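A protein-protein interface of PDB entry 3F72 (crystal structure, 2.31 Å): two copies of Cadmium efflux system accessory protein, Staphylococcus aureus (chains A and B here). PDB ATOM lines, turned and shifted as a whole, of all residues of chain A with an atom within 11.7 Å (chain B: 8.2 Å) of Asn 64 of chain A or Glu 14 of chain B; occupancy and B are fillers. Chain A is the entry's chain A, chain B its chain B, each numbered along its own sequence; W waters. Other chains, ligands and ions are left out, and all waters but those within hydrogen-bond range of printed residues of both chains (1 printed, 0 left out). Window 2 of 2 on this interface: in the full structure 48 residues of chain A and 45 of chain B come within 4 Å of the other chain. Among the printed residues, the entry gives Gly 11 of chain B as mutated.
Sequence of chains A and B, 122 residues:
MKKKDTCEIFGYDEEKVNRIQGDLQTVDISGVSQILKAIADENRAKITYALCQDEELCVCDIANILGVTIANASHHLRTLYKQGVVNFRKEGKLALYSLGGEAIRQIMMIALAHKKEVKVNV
No position is printed for both chains.
Ala 50 of chain A touches Ile 20 of chain B (CB to CG2, 3.8 Å).
Ile 20 of chain B touches Asp 54 of chain A.
Leu 57 of chain A touches Lys 16 of chain B.
Cys 60 of chain A touches Tyr 12 of chain B (CB to CE2, 3.3 Å).
OD1 of Asp 61 of chain A touches CE2 of Tyr 12 of chain B, at 3.7 Å.
Asp 61 of chain A touches Lys 16 of chain B (OD2 to CD, 3.9 Å).
Val 17 of chain B touches Asp 61 of chain A.
Asn 64 of chain A touches Val 17 of chain B (C to CG1, 3.7 Å).
CG1 of Val 17 of chain B touches N of Ile 65 of chain A (3.5 Å).
Ile 65 of chain A touches Ile 20 of chain B.
Water W1 bridges the side-chain amino group of Lys 16 of chain B (2.6 Å) and the side-chain carboxylate of Asp 54 of chain A (2.8 Å).
Hydrophobic or aromatic side chains of chain A that line the printed part of chain B: Ala 50, Leu 57 and Ile 65.
Along chain A the printed residues that touch a printed residue of chain B span positions 50 to 65.
Among the printed residues, Asp or Glu carboxylates within 4 Å of a Lys or Arg side-chain nitrogen of the other chain: Asp 54 of chain A with Arg 19 of chain B (2.6 Å).
The guanidinium group (NH1) of Arg 19 of chain B lies within salt-bridge range of the side-chain carboxylate (OD2) of Asp 54 of chain A (2.6 Å).
The side-chain hydroxyl (OH) of Tyr 12 of chain B lies within hydrogen-bond range of the side-chain sulfur (SG) of Cys 58 of chain A, 3.3 Å away.
The side-chain carboxylate (OD1) of Asp 61 of chain A sits close to the side-chain carboxylate (OD2) of Asp 13 of chain B (2.7 Å).
ND2 of Asn 64 of chain A lies within hydrogen-bond range of O of Tyr 12 of chain B (2.9 Å).
The side-chain carboxylate of Glu 14 of chain B sits at hydrogen-bond distance from the side-chain amide nitrogen of Asn 64 of chain A, 2.9 Å away.
The backbone carbonyl oxygen of Asn 64 of chain A sits at hydrogen-bond distance from the side-chain amide nitrogen of Gln 21 of chain B (3.3 Å).
The backbone carbonyl oxygen of Ile 65 of chain A is in hydrogen-bond range of the side-chain amide nitrogen of Gln 21 of chain B (2.9 Å).
Of the printed residues of chain B, Asp 61 of chain A touches Tyr 12 (3.7 Å), Asp 13 (2.7 Å), Lys 16 (3.9 Å) and Val 17 (3.9 Å).
No residue of chain A comes within 4 Å of Phe 10 of chain B.
No residue of chain A comes within 4 Å of Gly 11 of chain B.
Of chain A, only Asp 61 (2.7 Å) comes within 4 Å of Asp 13 of chain B.
Of chain A, only Asn 64 comes within 4 Å of Glu 14 of chain B.
No residue of chain A comes within 4 Å of Glu 15 of chain B.
Of chain A, only Asp 61 (3.9 Å), Asn 64 (3.7 Å) and Ile 65 (3.5 Å) come within 4 Å of Val 17 of chain B.
No residue of chain A comes within 4 Å of Asn 18 of chain B.
Of the printed residues of chain A, Gln 21 of chain B touches Asn 64 and Ile 65.
The nearest residue of chain B that does not touch Asn 64 of chain A is Asp 13 of chain B (5.1 Å).
O of Leu 57 of chain A lies within hydrogen-bond range of N of Tyr 97 of chain A (2.9 Å).
The backbone NH (N) of Cys 58 of chain A lies within hydrogen-bond range of the side-chain carboxylate (OD2) of Asp 61 of chain A (3.3 Å).
The side-chain carboxylate of Glu 14 of chain B is in hydrogen-bond range of the backbone NH of Tyr 12 of chain B (2.5 Å).
O of Glu 14 of chain B lies close to ND2 of Asn 18 of chain B.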
ATOM      1  N   ASN A  43     -29.396  -1.397  12.962  1.00  0.00           N
ATOM      2  CA  ASN A  43     -28.517  -0.227  12.663  1.00  0.00           C
ATOM      3  C   ASN A  43     -27.395  -0.593  11.715  1.00  0.00           C
ATOM      4  O   ASN A  43     -27.141   0.122  10.677  1.00  0.00           O
ATOM      5  CB  ASN A  43     -28.038   0.392  13.999  1.00  0.00           C
ATOM      6  CG  ASN A  43     -29.199   1.218  14.765  1.00  0.00           C
ATOM      7  OD1 ASN A  43     -30.061   1.777  14.153  1.00  0.00           O
ATOM      8  ND2 ASN A  43     -29.118   1.302  16.067  1.00  0.00           N
ATOM      9  N   LYS A  46     -28.989  -0.718   8.129  1.00  0.00           N
ATOM     10  CA  LYS A  46     -28.977   0.777   7.797  1.00  0.00           C
ATOM     11  C   LYS A  46     -27.578   1.276   7.387  1.00  0.00           C
ATOM     12  O   LYS A  46     -27.409   1.877   6.393  1.00  0.00           O
ATOM     13  CB  LYS A  46     -29.651   1.618   8.933  1.00  0.00           C
ATOM     14  CG  LYS A  46     -31.184   1.177   9.226  1.00  0.00           C
ATOM     15  CD  LYS A  46     -32.038   2.318   9.735  1.00  0.00           C
ATOM     16  CE  LYS A  46     -33.260   1.924  10.641  1.00  0.00           C
ATOM     17  NZ  LYS A  46     -32.728   1.568  12.069  1.00  0.00           N
ATOM     18  N   ILE A  47     -26.539   0.949   8.116  1.00  0.00           N
ATOM     19  CA  ILE A  47     -25.267   1.409   7.639  1.00  0.00           C
ATOM     20  C   ILE A  47     -24.870   0.834   6.284  1.00  0.00           C
ATOM     21  O   ILE A  47     -24.320   1.591   5.421  1.00  0.00           O
ATOM     22  CB  ILE A  47     -24.128   1.178   8.638  1.00  0.00           C
ATOM     23  CG1 ILE A  47     -24.425   1.918   9.917  1.00  0.00           C
ATOM     24  CG2 ILE A  47     -22.826   1.713   8.092  1.00  0.00           C
ATOM     25  CD1 ILE A  47     -23.618   1.407  11.116  1.00  0.00           C
ATOM     26  N   ALA A  50     -26.874   2.508   3.498  1.00  0.00           N
ATOM     27  CA  ALA A  50     -26.344   3.833   3.158  1.00  0.00           C
ATOM     28  C   ALA A  50     -25.057   3.756   2.292  1.00  0.00           C
ATOM     29  O   ALA A  50     -24.865   4.558   1.358  1.00  0.00           O
ATOM     30  CB  ALA A  50     -26.109   4.679   4.495  1.00  0.00           C
ATOM     31  N   ASP A  54     -24.012   5.892  -1.240  1.00  0.00           N
ATOM     32  CA  ASP A  54     -22.903   6.900  -1.320  1.00  0.00           C
ATOM     33  C   ASP A  54     -21.570   6.223  -1.043  1.00  0.00           C
ATOM     34  O   ASP A  54     -21.508   5.374  -0.181  1.00  0.00           O
ATOM     35  CB  ASP A  54     -23.098   7.954  -0.234  1.00  0.00           C
ATOM     36  CG  ASP A  54     -24.089   9.017  -0.618  1.00  0.00           C
ATOM     37  OD1 ASP A  54     -23.629  10.176  -0.824  1.00  0.00           O
ATOM     38  OD2 ASP A  54     -25.319   8.733  -0.683  1.00  0.00           O
ATOM     39  N   LEU A  57     -18.698   7.723   3.876  1.00  0.00           N
ATOM     40  CA  LEU A  57     -19.393   8.401   4.946  1.00  0.00           C
ATOM     41  C   LEU A  57     -18.436   8.470   6.146  1.00  0.00           C
ATOM     42  O   LEU A  57     -17.580   7.572   6.298  1.00  0.00           O
ATOM     43  CB  LEU A  57     -20.697   7.657   5.239  1.00  0.00           C
ATOM     44  CG  LEU A  57     -21.778   7.811   4.126  1.00  0.00           C
ATOM     45  CD1 LEU A  57     -23.006   6.981   4.372  1.00  0.00           C
ATOM     46  CD2 LEU A  57     -22.183   9.255   3.792  1.00  0.00           C
ATOM     47  N   CYS A  58     -18.488   9.522   6.988  1.00  0.00           N
ATOM     48  CA  CYS A  58     -17.536   9.477   8.163  1.00  0.00           C
ATOM     49  C   CYS A  58     -18.332   8.976   9.353  1.00  0.00           C
ATOM     50  O   CYS A  58     -19.556   8.796   9.235  1.00  0.00           O
ATOM     51  CB  CYS A  58     -16.911  10.854   8.469  1.00  0.00           C
ATOM     52  SG  CYS A  58     -18.075  12.135   8.693  1.00  0.00           S
ATOM     53  N   VAL A  59     -17.733   8.776  10.504  1.00  0.00           N
ATOM     54  CA  VAL A  59     -18.588   8.188  11.532  1.00  0.00           C
ATOM     55  C   VAL A  59     -19.710   9.090  11.959  1.00  0.00           C
ATOM     56  O   VAL A  59     -20.815   8.605  12.224  1.00  0.00           O
ATOM     57  CB  VAL A  59     -17.773   7.599  12.770  1.00  0.00           C
ATOM     58  CG1 VAL A  59     -16.878   8.705  13.376  1.00  0.00           C
ATOM     59  CG2 VAL A  59     -18.757   7.035  13.844  1.00  0.00           C
ATOM     60  N   CYS A  60     -19.478  10.413  12.005  1.00  0.00           N
ATOM     61  CA  CYS A  60     -20.484  11.395  12.383  1.00  0.00           C
ATOM     62  C   CYS A  60     -21.727  11.419  11.420  1.00  0.00           C
ATOM     63  O   CYS A  60     -22.825  11.560  11.922  1.00  0.00           O
ATOM     64  CB  CYS A  60     -19.838  12.729  12.347  1.00  0.00           C
ATOM     65  SG  CYS A  60     -18.330  12.896  13.395  1.00  0.00           S
ATOM     66  N   ASP A  61     -21.553  11.330  10.083  1.00  0.00           N
ATOM     67  CA  ASP A  61     -22.655  11.100   9.143  1.00  0.00           C
ATOM     68  C   ASP A  61     -23.540   9.942   9.592  1.00  0.00           C
ATOM     69  O   ASP A  61     -24.770  10.077   9.825  1.00  0.00           O
ATOM     70  CB  ASP A  61     -22.100  10.710   7.828  1.00  0.00           C
ATOM     71  CG  ASP A  61     -21.532  11.858   7.020  1.00  0.00           C
ATOM     72  OD1 ASP A  61     -21.731  13.050   7.310  1.00  0.00           O
ATOM     73  OD2 ASP A  61     -20.886  11.494   6.001  1.00  0.00           O
ATOM     74  N   ILE A  62     -22.876   8.822   9.791  1.00  0.00           N
ATOM     75  CA  ILE A  62     -23.458   7.607  10.403  1.00  0.00           C
ATOM     76  C   ILE A  62     -24.072   7.826  11.769  1.00  0.00           C
ATOM     77  O   ILE A  62     -25.262   7.546  11.931  1.00  0.00           O
ATOM     78  CB  ILE A  62     -22.417   6.418  10.363  1.00  0.00           C
ATOM     79  CG1 ILE A  62     -22.290   6.013   8.883  1.00  0.00           C
ATOM     80  CG2 ILE A  62     -22.997   5.131  11.110  1.00  0.00           C
ATOM     81  CD1 ILE A  62     -20.907   5.762   8.378  1.00  0.00           C
ATOM     82  N   ALA A  63     -23.348   8.390  12.762  1.00  0.00           N
ATOM     83  CA  ALA A  63     -24.120   8.730  13.966  1.00  0.00           C
ATOM     84  C   ALA A  63     -25.439   9.531  13.630  1.00  0.00           C
ATOM     85  O   ALA A  63     -26.536   9.253  14.163  1.00  0.00           O
ATOM     86  CB  ALA A  63     -23.332   9.480  14.868  1.00  0.00           C
ATOM     87  N   ASN A  64     -25.321  10.517  12.732  1.00  0.00           N
ATOM     88  CA  ASN A  64     -26.438  11.408  12.464  1.00  0.00           C
ATOM     89  C   ASN A  64     -27.483  10.726  11.547  1.00  0.00           C
ATOM     90  O   ASN A  64     -28.665  10.782  11.895  1.00  0.00           O
ATOM     91  CB  ASN A  64     -25.925  12.689  11.853  1.00  0.00           C
ATOM     92  CG  ASN A  64     -26.783  13.916  12.194  1.00  0.00           C
ATOM     93  OD1 ASN A  64     -27.772  13.942  13.046  1.00  0.00           O
ATOM     94  ND2 ASN A  64     -26.400  14.973  11.485  1.00  0.00           N
ATOM     95  N   ILE A  65     -27.092  10.092  10.422  1.00  0.00           N
ATOM     96  CA  ILE A  65     -28.062   9.161   9.687  1.00  0.00           C
ATOM     97  C   ILE A  65     -28.912   8.290  10.626  1.00  0.00           C
ATOM     98  O   ILE A  65     -30.123   8.346  10.583  1.00  0.00           O
ATOM     99  CB  ILE A  65     -27.389   8.261   8.658  1.00  0.00           C
ATOM    100  CG1 ILE A  65     -26.967   9.074   7.471  1.00  0.00           C
ATOM    101  CG2 ILE A  65     -28.393   7.169   8.135  1.00  0.00           C
ATOM    102  CD1 ILE A  65     -25.793   8.576   6.898  1.00  0.00           C
ATOM    103  N   LEU A  66     -28.289   7.581  11.570  1.00  0.00           N
ATOM    104  CA  LEU A  66     -29.031   6.669  12.475  1.00  0.00           C
ATOM    105  C   LEU A  66     -29.727   7.265  13.614  1.00  0.00           C
ATOM    106  O   LEU A  66     -30.564   6.569  14.306  1.00  0.00           O
ATOM    107  CB  LEU A  66     -28.077   5.610  13.079  1.00  0.00           C
ATOM    108  CG  LEU A  66     -27.284   4.692  12.071  1.00  0.00           C
ATOM    109  CD1 LEU A  66     -26.303   3.831  12.932  1.00  0.00           C
ATOM    110  CD2 LEU A  66     -28.223   3.749  11.296  1.00  0.00           C
ATOM    111  N   GLY A  67     -29.295   8.490  13.953  1.00  0.00           N
ATOM    112  CA  GLY A  67     -29.745   9.157  15.157  1.00  0.00           C
ATOM    113  C   GLY A  67     -29.208   8.506  16.373  1.00  0.00           C
ATOM    114  O   GLY A  67     -29.957   8.349  17.383  1.00  0.00           O
ATOM    115  N   VAL A  68     -27.884   8.131  16.332  1.00  0.00           N
ATOM    116  CA  VAL A  68     -27.266   7.516  17.536  1.00  0.00           C
ATOM    117  C   VAL A  68     -25.978   8.327  18.041  1.00  0.00           C
ATOM    118  O   VAL A  68     -25.402   9.124  17.303  1.00  0.00           O
ATOM    119  CB  VAL A  68     -26.912   5.959  17.328  1.00  0.00           C
ATOM    120  CG1 VAL A  68     -28.160   5.056  17.367  1.00  0.00           C
ATOM    121  CG2 VAL A  68     -26.065   5.828  16.095  1.00  0.00           C
ATOM    122  N   THR A  69     -25.580   8.136  19.301  1.00  0.00           N
ATOM    123  CA  THR A  69     -24.254   8.689  19.729  1.00  0.00           C
ATOM    124  C   THR A  69     -23.176   8.179  18.757  1.00  0.00           C
ATOM    125  O   THR A  69     -23.447   7.157  18.046  1.00  0.00           O
ATOM    126  CB  THR A  69     -23.918   8.308  21.165  1.00  0.00           C
ATOM    127  OG1 THR A  69     -23.747   6.890  21.296  1.00  0.00           O
ATOM    128  CG2 THR A  69     -25.042   8.831  22.068  1.00  0.00           C
ATOM    129  N   ILE A  70     -22.052   8.901  18.671  1.00  0.00           N
ATOM    130  CA  ILE A  70     -20.852   8.509  17.921  1.00  0.00           C
ATOM    131  C   ILE A  70     -20.228   7.208  18.519  1.00  0.00           C
ATOM    132  O   ILE A  70     -19.662   6.383  17.792  1.00  0.00           O
ATOM    133  CB  ILE A  70     -19.669   9.645  18.034  1.00  0.00           C
ATOM    134  CG1 ILE A  70     -20.077  11.062  17.535  1.00  0.00           C
ATOM    135  CG2 ILE A  70     -18.261   9.159  17.528  1.00  0.00           C
ATOM    136  CD1 ILE A  70     -20.919  11.075  16.309  1.00  0.00           C
ATOM    137  N   ALA A  71     -20.301   7.050  19.837  1.00  0.00           N
ATOM    138  CA  ALA A  71     -19.770   5.854  20.429  1.00  0.00           C
ATOM    139  C   ALA A  71     -20.596   4.653  19.880  1.00  0.00           C
ATOM    140  O   ALA A  71     -20.051   3.660  19.470  1.00  0.00           O
ATOM    141  CB  ALA A  71     -19.832   5.958  21.943  1.00  0.00           C
ATOM    142  N   ASN A  72     -21.899   4.789  19.814  1.00  0.00           N
ATOM    143  CA  ASN A  72     -22.775   3.764  19.237  1.00  0.00           C
ATOM    144  C   ASN A  72     -22.404   3.472  17.824  1.00  0.00           C
ATOM    145  O   ASN A  72     -22.191   2.293  17.470  1.00  0.00           O
ATOM    146  CB  ASN A  72     -24.199   4.172  19.325  1.00  0.00           C
ATOM    147  CG  ASN A  72     -25.172   2.986  19.017  1.00  0.00           C
ATOM    148  OD1 ASN A  72     -26.060   3.090  18.194  1.00  0.00           O
ATOM    149  ND2 ASN A  72     -24.984   1.871  19.704  1.00  0.00           N
ATOM    150  N   ALA A  73     -22.198   4.530  17.044  1.00  0.00           N
ATOM    151  CA  ALA A  73     -21.760   4.375  15.674  1.00  0.00           C
ATOM    152  C   ALA A  73     -20.389   3.713  15.442  1.00  0.00           C
ATOM    153  O   ALA A  73     -20.208   2.886  14.501  1.00  0.00           O
ATOM    154  CB  ALA A  73     -21.913   5.712  14.878  1.00  0.00           C
ATOM    155  N   SER A  74     -19.377   4.129  16.227  1.00  0.00           N
ATOM    156  CA  SER A  74     -18.088   3.465  16.153  1.00  0.00           C
ATOM    157  C   SER A  74     -18.173   2.003  16.482  1.00  0.00           C
ATOM    158  O   SER A  74     -17.468   1.246  15.905  1.00  0.00           O
ATOM    159  CB  SER A  74     -17.146   4.060  17.173  1.00  0.00           C
ATOM    160  OG  SER A  74     -17.060   5.440  16.972  1.00  0.00           O
ATOM    161  N   HIS A  76     -20.671  -0.109  16.049  1.00  0.00           N
ATOM    162  CA  HIS A  76     -21.269  -0.756  14.902  1.00  0.00           C
ATOM    163  C   HIS A  76     -20.321  -0.818  13.766  1.00  0.00           C
ATOM    164  O   HIS A  76     -20.380  -1.779  13.010  1.00  0.00           O
ATOM    165  CB  HIS A  76     -22.599  -0.124  14.441  1.00  0.00           C
ATOM    166  CG  HIS A  76     -23.763  -0.486  15.317  1.00  0.00           C
ATOM    167  ND1 HIS A  76     -24.653   0.444  15.774  1.00  0.00           N
ATOM    168  CD2 HIS A  76     -24.146  -1.674  15.855  1.00  0.00           C
ATOM    169  CE1 HIS A  76     -25.543  -0.150  16.564  1.00  0.00           C
ATOM    170  NE2 HIS A  76     -25.266  -1.441  16.614  1.00  0.00           N
ATOM    171  N   LEU A  77     -19.467   0.184  13.620  1.00  0.00           N
ATOM    172  CA  LEU A  77     -18.612   0.172  12.476  1.00  0.00           C
ATOM    173  C   LEU A  77     -17.424  -0.796  12.593  1.00  0.00           C
ATOM    174  O   LEU A  77     -16.838  -1.291  11.568  1.00  0.00           O
ATOM    175  CB  LEU A  77     -18.146   1.591  12.149  1.00  0.00           C
ATOM    176  CG  LEU A  77     -19.112   2.479  11.319  1.00  0.00           C
ATOM    177  CD1 LEU A  77     -18.724   3.987  11.395  1.00  0.00           C
ATOM    178  CD2 LEU A  77     -19.201   2.049   9.796  1.00  0.00           C
ATOM    179  N   TYR A  97     -15.497   5.820   5.320  1.00  0.00           N
ATOM    180  CA  TYR A  97     -15.892   4.424   5.277  1.00  0.00           C
ATOM    181  C   TYR A  97     -16.631   4.135   4.035  1.00  0.00           C
ATOM    182  O   TYR A  97     -17.457   4.915   3.588  1.00  0.00           O
ATOM    183  CB  TYR A  97     -16.797   4.046   6.459  1.00  0.00           C
ATOM    184  CG  TYR A  97     -16.110   4.079   7.779  1.00  0.00           C
ATOM    185  CD1 TYR A  97     -15.590   2.941   8.324  1.00  0.00           C
ATOM    186  CD2 TYR A  97     -15.990   5.282   8.492  1.00  0.00           C
ATOM    187  CE1 TYR A  97     -14.956   2.979   9.538  1.00  0.00           C
ATOM    188  CE2 TYR A  97     -15.373   5.334   9.680  1.00  0.00           C
ATOM    189  CZ  TYR A  97     -14.847   4.204  10.217  1.00  0.00           C
ATOM    190  OH  TYR A  97     -14.246   4.252  11.474  1.00  0.00           O
ATOM    191  N   PHE B  10     -24.545  25.083  11.382  1.00  0.00           N
ATOM    192  CA  PHE B  10     -25.937  24.813  11.622  1.00  0.00           C
ATOM    193  C   PHE B  10     -26.024  23.685  12.723  1.00  0.00           C
ATOM    194  O   PHE B  10     -26.244  23.994  13.981  1.00  0.00           O
ATOM    195  CB  PHE B  10     -26.610  24.470  10.224  1.00  0.00           C
ATOM    196  CG  PHE B  10     -27.981  23.935  10.369  1.00  0.00           C
ATOM    197  CD1 PHE B  10     -29.021  24.766  10.844  1.00  0.00           C
ATOM    198  CD2 PHE B  10     -28.220  22.578  10.226  1.00  0.00           C
ATOM    199  CE1 PHE B  10     -30.298  24.285  11.110  1.00  0.00           C
ATOM    200  CE2 PHE B  10     -29.572  22.048  10.498  1.00  0.00           C
ATOM    201  CZ  PHE B  10     -30.589  22.919  10.931  1.00  0.00           C
ATOM    202  N   GLY B  11     -25.782  22.411  12.220  1.00  0.00           N
ATOM    203  CA  GLY B  11     -25.733  21.082  12.862  1.00  0.00           C
ATOM    204  C   GLY B  11     -24.638  20.281  12.106  1.00  0.00           C
ATOM    205  O   GLY B  11     -23.533  20.817  11.880  1.00  0.00           O
ATOM    206  N   TYR B  12     -24.859  19.036  11.661  1.00  0.00           N
ATOM    207  CA  TYR B  12     -23.787  18.375  10.864  1.00  0.00           C
ATOM    208  C   TYR B  12     -24.112  17.565   9.605  1.00  0.00           C
ATOM    209  O   TYR B  12     -24.653  16.424   9.668  1.00  0.00           O
ATOM    210  CB  TYR B  12     -22.959  17.450  11.764  1.00  0.00           C
ATOM    211  CG  TYR B  12     -21.738  16.895  11.099  1.00  0.00           C
ATOM    212  CD1 TYR B  12     -20.684  17.710  10.803  1.00  0.00           C
ATOM    213  CD2 TYR B  12     -21.647  15.572  10.720  1.00  0.00           C
ATOM    214  CE1 TYR B  12     -19.515  17.201  10.199  1.00  0.00           C
ATOM    215  CE2 TYR B  12     -20.514  15.069  10.120  1.00  0.00           C
ATOM    216  CZ  TYR B  12     -19.448  15.880   9.879  1.00  0.00           C
ATOM    217  OH  TYR B  12     -18.302  15.429   9.256  1.00  0.00           O
ATOM    218  N   ASP B  13     -23.597  18.058   8.483  1.00  0.00           N
ATOM    219  CA  ASP B  13     -23.903  17.482   7.203  1.00  0.00           C
ATOM    220  C   ASP B  13     -25.382  17.227   6.994  1.00  0.00           C
ATOM    221  O   ASP B  13     -25.722  16.170   6.547  1.00  0.00           O
ATOM    222  CB  ASP B  13     -23.168  16.168   6.969  1.00  0.00           C
ATOM    223  CG  ASP B  13     -21.924  16.348   6.161  1.00  0.00           C
ATOM    224  OD1 ASP B  13     -21.699  17.477   5.719  1.00  0.00           O
ATOM    225  OD2 ASP B  13     -21.135  15.377   6.016  1.00  0.00           O
ATOM    226  N   GLU B  14     -26.221  18.177   7.276  1.00  0.00           N
ATOM    227  CA  GLU B  14     -27.629  17.919   7.468  1.00  0.00           C
ATOM    228  C   GLU B  14     -28.460  17.476   6.288  1.00  0.00           C
ATOM    229  O   GLU B  14     -29.534  16.778   6.474  1.00  0.00           O
ATOM    230  CB  GLU B  14     -28.293  19.148   8.133  1.00  0.00           C
ATOM    231  CG  GLU B  14     -27.671  19.333   9.551  1.00  0.00           C
ATOM    232  CD  GLU B  14     -27.899  18.084  10.423  1.00  0.00           C
ATOM    233  OE1 GLU B  14     -28.962  17.410  10.187  1.00  0.00           O
ATOM    234  OE2 GLU B  14     -27.019  17.796  11.317  1.00  0.00           O
ATOM    235  N   GLU B  15     -28.038  17.966   5.109  1.00  0.00           N
ATOM    236  CA  GLU B  15     -28.820  17.772   3.919  1.00  0.00           C
ATOM    237  C   GLU B  15     -28.396  16.445   3.322  1.00  0.00           C
ATOM    238  O   GLU B  15     -29.230  15.756   2.755  1.00  0.00           O
ATOM    239  CB  GLU B  15     -28.658  18.922   2.909  1.00  0.00           C
ATOM    240  CG  GLU B  15     -27.505  18.702   1.949  1.00  0.00           C
ATOM    241  CD  GLU B  15     -27.418  19.735   0.817  1.00  0.00           C
ATOM    242  OE1 GLU B  15     -26.241  20.023   0.463  1.00  0.00           O
ATOM    243  OE2 GLU B  15     -28.479  20.247   0.287  1.00  0.00           O
ATOM    244  N   LYS B  16     -27.111  16.106   3.459  1.00  0.00           N
ATOM    245  CA  LYS B  16     -26.666  14.782   3.129  1.00  0.00           C
ATOM    246  C   LYS B  16     -27.237  13.724   4.077  1.00  0.00           C
ATOM    247  O   LYS B  16     -27.902  12.722   3.627  1.00  0.00           O
ATOM    248  CB  LYS B  16     -25.201  14.666   3.175  1.00  0.00           C
ATOM    249  CG  LYS B  16     -24.838  13.215   3.202  1.00  0.00           C
ATOM    250  CD  LYS B  16     -23.369  13.041   3.372  1.00  0.00           C
ATOM    251  CE  LYS B  16     -22.696  13.618   2.196  1.00  0.00           C
ATOM    252  NZ  LYS B  16     -21.345  13.071   2.113  1.00  0.00           N
ATOM    253  N   VAL B  17     -27.018  13.907   5.381  1.00  0.00           N
ATOM    254  CA  VAL B  17     -27.806  13.067   6.346  1.00  0.00           C
ATOM    255  C   VAL B  17     -29.293  12.872   5.958  1.00  0.00           C
ATOM    256  O   VAL B  17     -29.840  11.776   6.008  1.00  0.00           O
ATOM    257  CB  VAL B  17     -27.621  13.522   7.828  1.00  0.00           C
ATOM    258  CG1 VAL B  17     -28.527  12.792   8.712  1.00  0.00           C
ATOM    259  CG2 VAL B  17     -26.206  13.311   8.187  1.00  0.00           C
ATOM    260  N   ASN B  18     -29.942  13.972   5.628  1.00  0.00           N
ATOM    261  CA  ASN B  18     -31.355  14.012   5.374  1.00  0.00           C
ATOM    262  C   ASN B  18     -31.812  13.340   4.136  1.00  0.00           C
ATOM    263  O   ASN B  18     -32.895  12.737   4.137  1.00  0.00           O
ATOM    264  CB  ASN B  18     -31.756  15.431   5.147  1.00  0.00           C
ATOM    265  CG  ASN B  18     -32.967  15.745   5.860  1.00  0.00           C
ATOM    266  OD1 ASN B  18     -34.101  15.533   5.357  1.00  0.00           O
ATOM    267  ND2 ASN B  18     -32.775  16.227   7.090  1.00  0.00           N
ATOM    268  N   ARG B  19     -31.001  13.508   3.090  1.00  0.00           N
ATOM    269  CA  ARG B  19     -31.124  12.796   1.874  1.00  0.00           C
ATOM    270  C   ARG B  19     -31.138  11.302   2.160  1.00  0.00           C
ATOM    271  O   ARG B  19     -32.119  10.623   1.942  1.00  0.00           O
ATOM    272  CB  ARG B  19     -29.908  13.071   1.006  1.00  0.00           C
ATOM    273  CG  ARG B  19     -30.110  12.470  -0.366  1.00  0.00           C
ATOM    274  CD  ARG B  19     -28.981  12.693  -1.343  1.00  0.00           C
ATOM    275  NE  ARG B  19     -27.582  12.771  -0.831  1.00  0.00           N
ATOM    276  CZ  ARG B  19     -26.675  11.808  -0.900  1.00  0.00           C
ATOM    277  NH1 ARG B  19     -26.992  10.611  -1.364  1.00  0.00           N
ATOM    278  NH2 ARG B  19     -25.459  12.036  -0.488  1.00  0.00           N
ATOM    279  N   ILE B  20     -29.999  10.805   2.601  1.00  0.00           N
ATOM    280  CA  ILE B  20     -29.843   9.420   3.041  1.00  0.00           C
ATOM    281  C   ILE B  20     -30.902   8.893   4.017  1.00  0.00           C
ATOM    282  O   ILE B  20     -31.348   7.790   3.855  1.00  0.00           O
ATOM    283  CB  ILE B  20     -28.446   9.172   3.541  1.00  0.00           C
ATOM    284  CG1 ILE B  20     -27.460   9.471   2.405  1.00  0.00           C
ATOM    285  CG2 ILE B  20     -28.308   7.743   3.972  1.00  0.00           C
ATOM    286  CD1 ILE B  20     -26.049   9.654   2.827  1.00  0.00           C
ATOM    287  N   GLN B  21     -31.362   9.669   4.976  1.00  0.00           N
ATOM    288  CA  GLN B  21     -32.480   9.166   5.798  1.00  0.00           C
ATOM    289  C   GLN B  21     -33.730   8.905   5.011  1.00  0.00           C
ATOM    290  O   GLN B  21     -34.565   8.046   5.422  1.00  0.00           O
ATOM    291  CB  GLN B  21     -32.824  10.116   6.934  1.00  0.00           C
ATOM    292  CG  GLN B  21     -31.564  10.378   7.894  1.00  0.00           C
ATOM    293  CD  GLN B  21     -31.941  11.278   9.034  1.00  0.00           C
ATOM    294  OE1 GLN B  21     -32.692  12.250   8.819  1.00  0.00           O
ATOM    295  NE2 GLN B  21     -31.558  10.903  10.267  1.00  0.00           N
HETATM  296  O   HOH W   1     -21.488  10.832   0.832  1.00  0.00           O
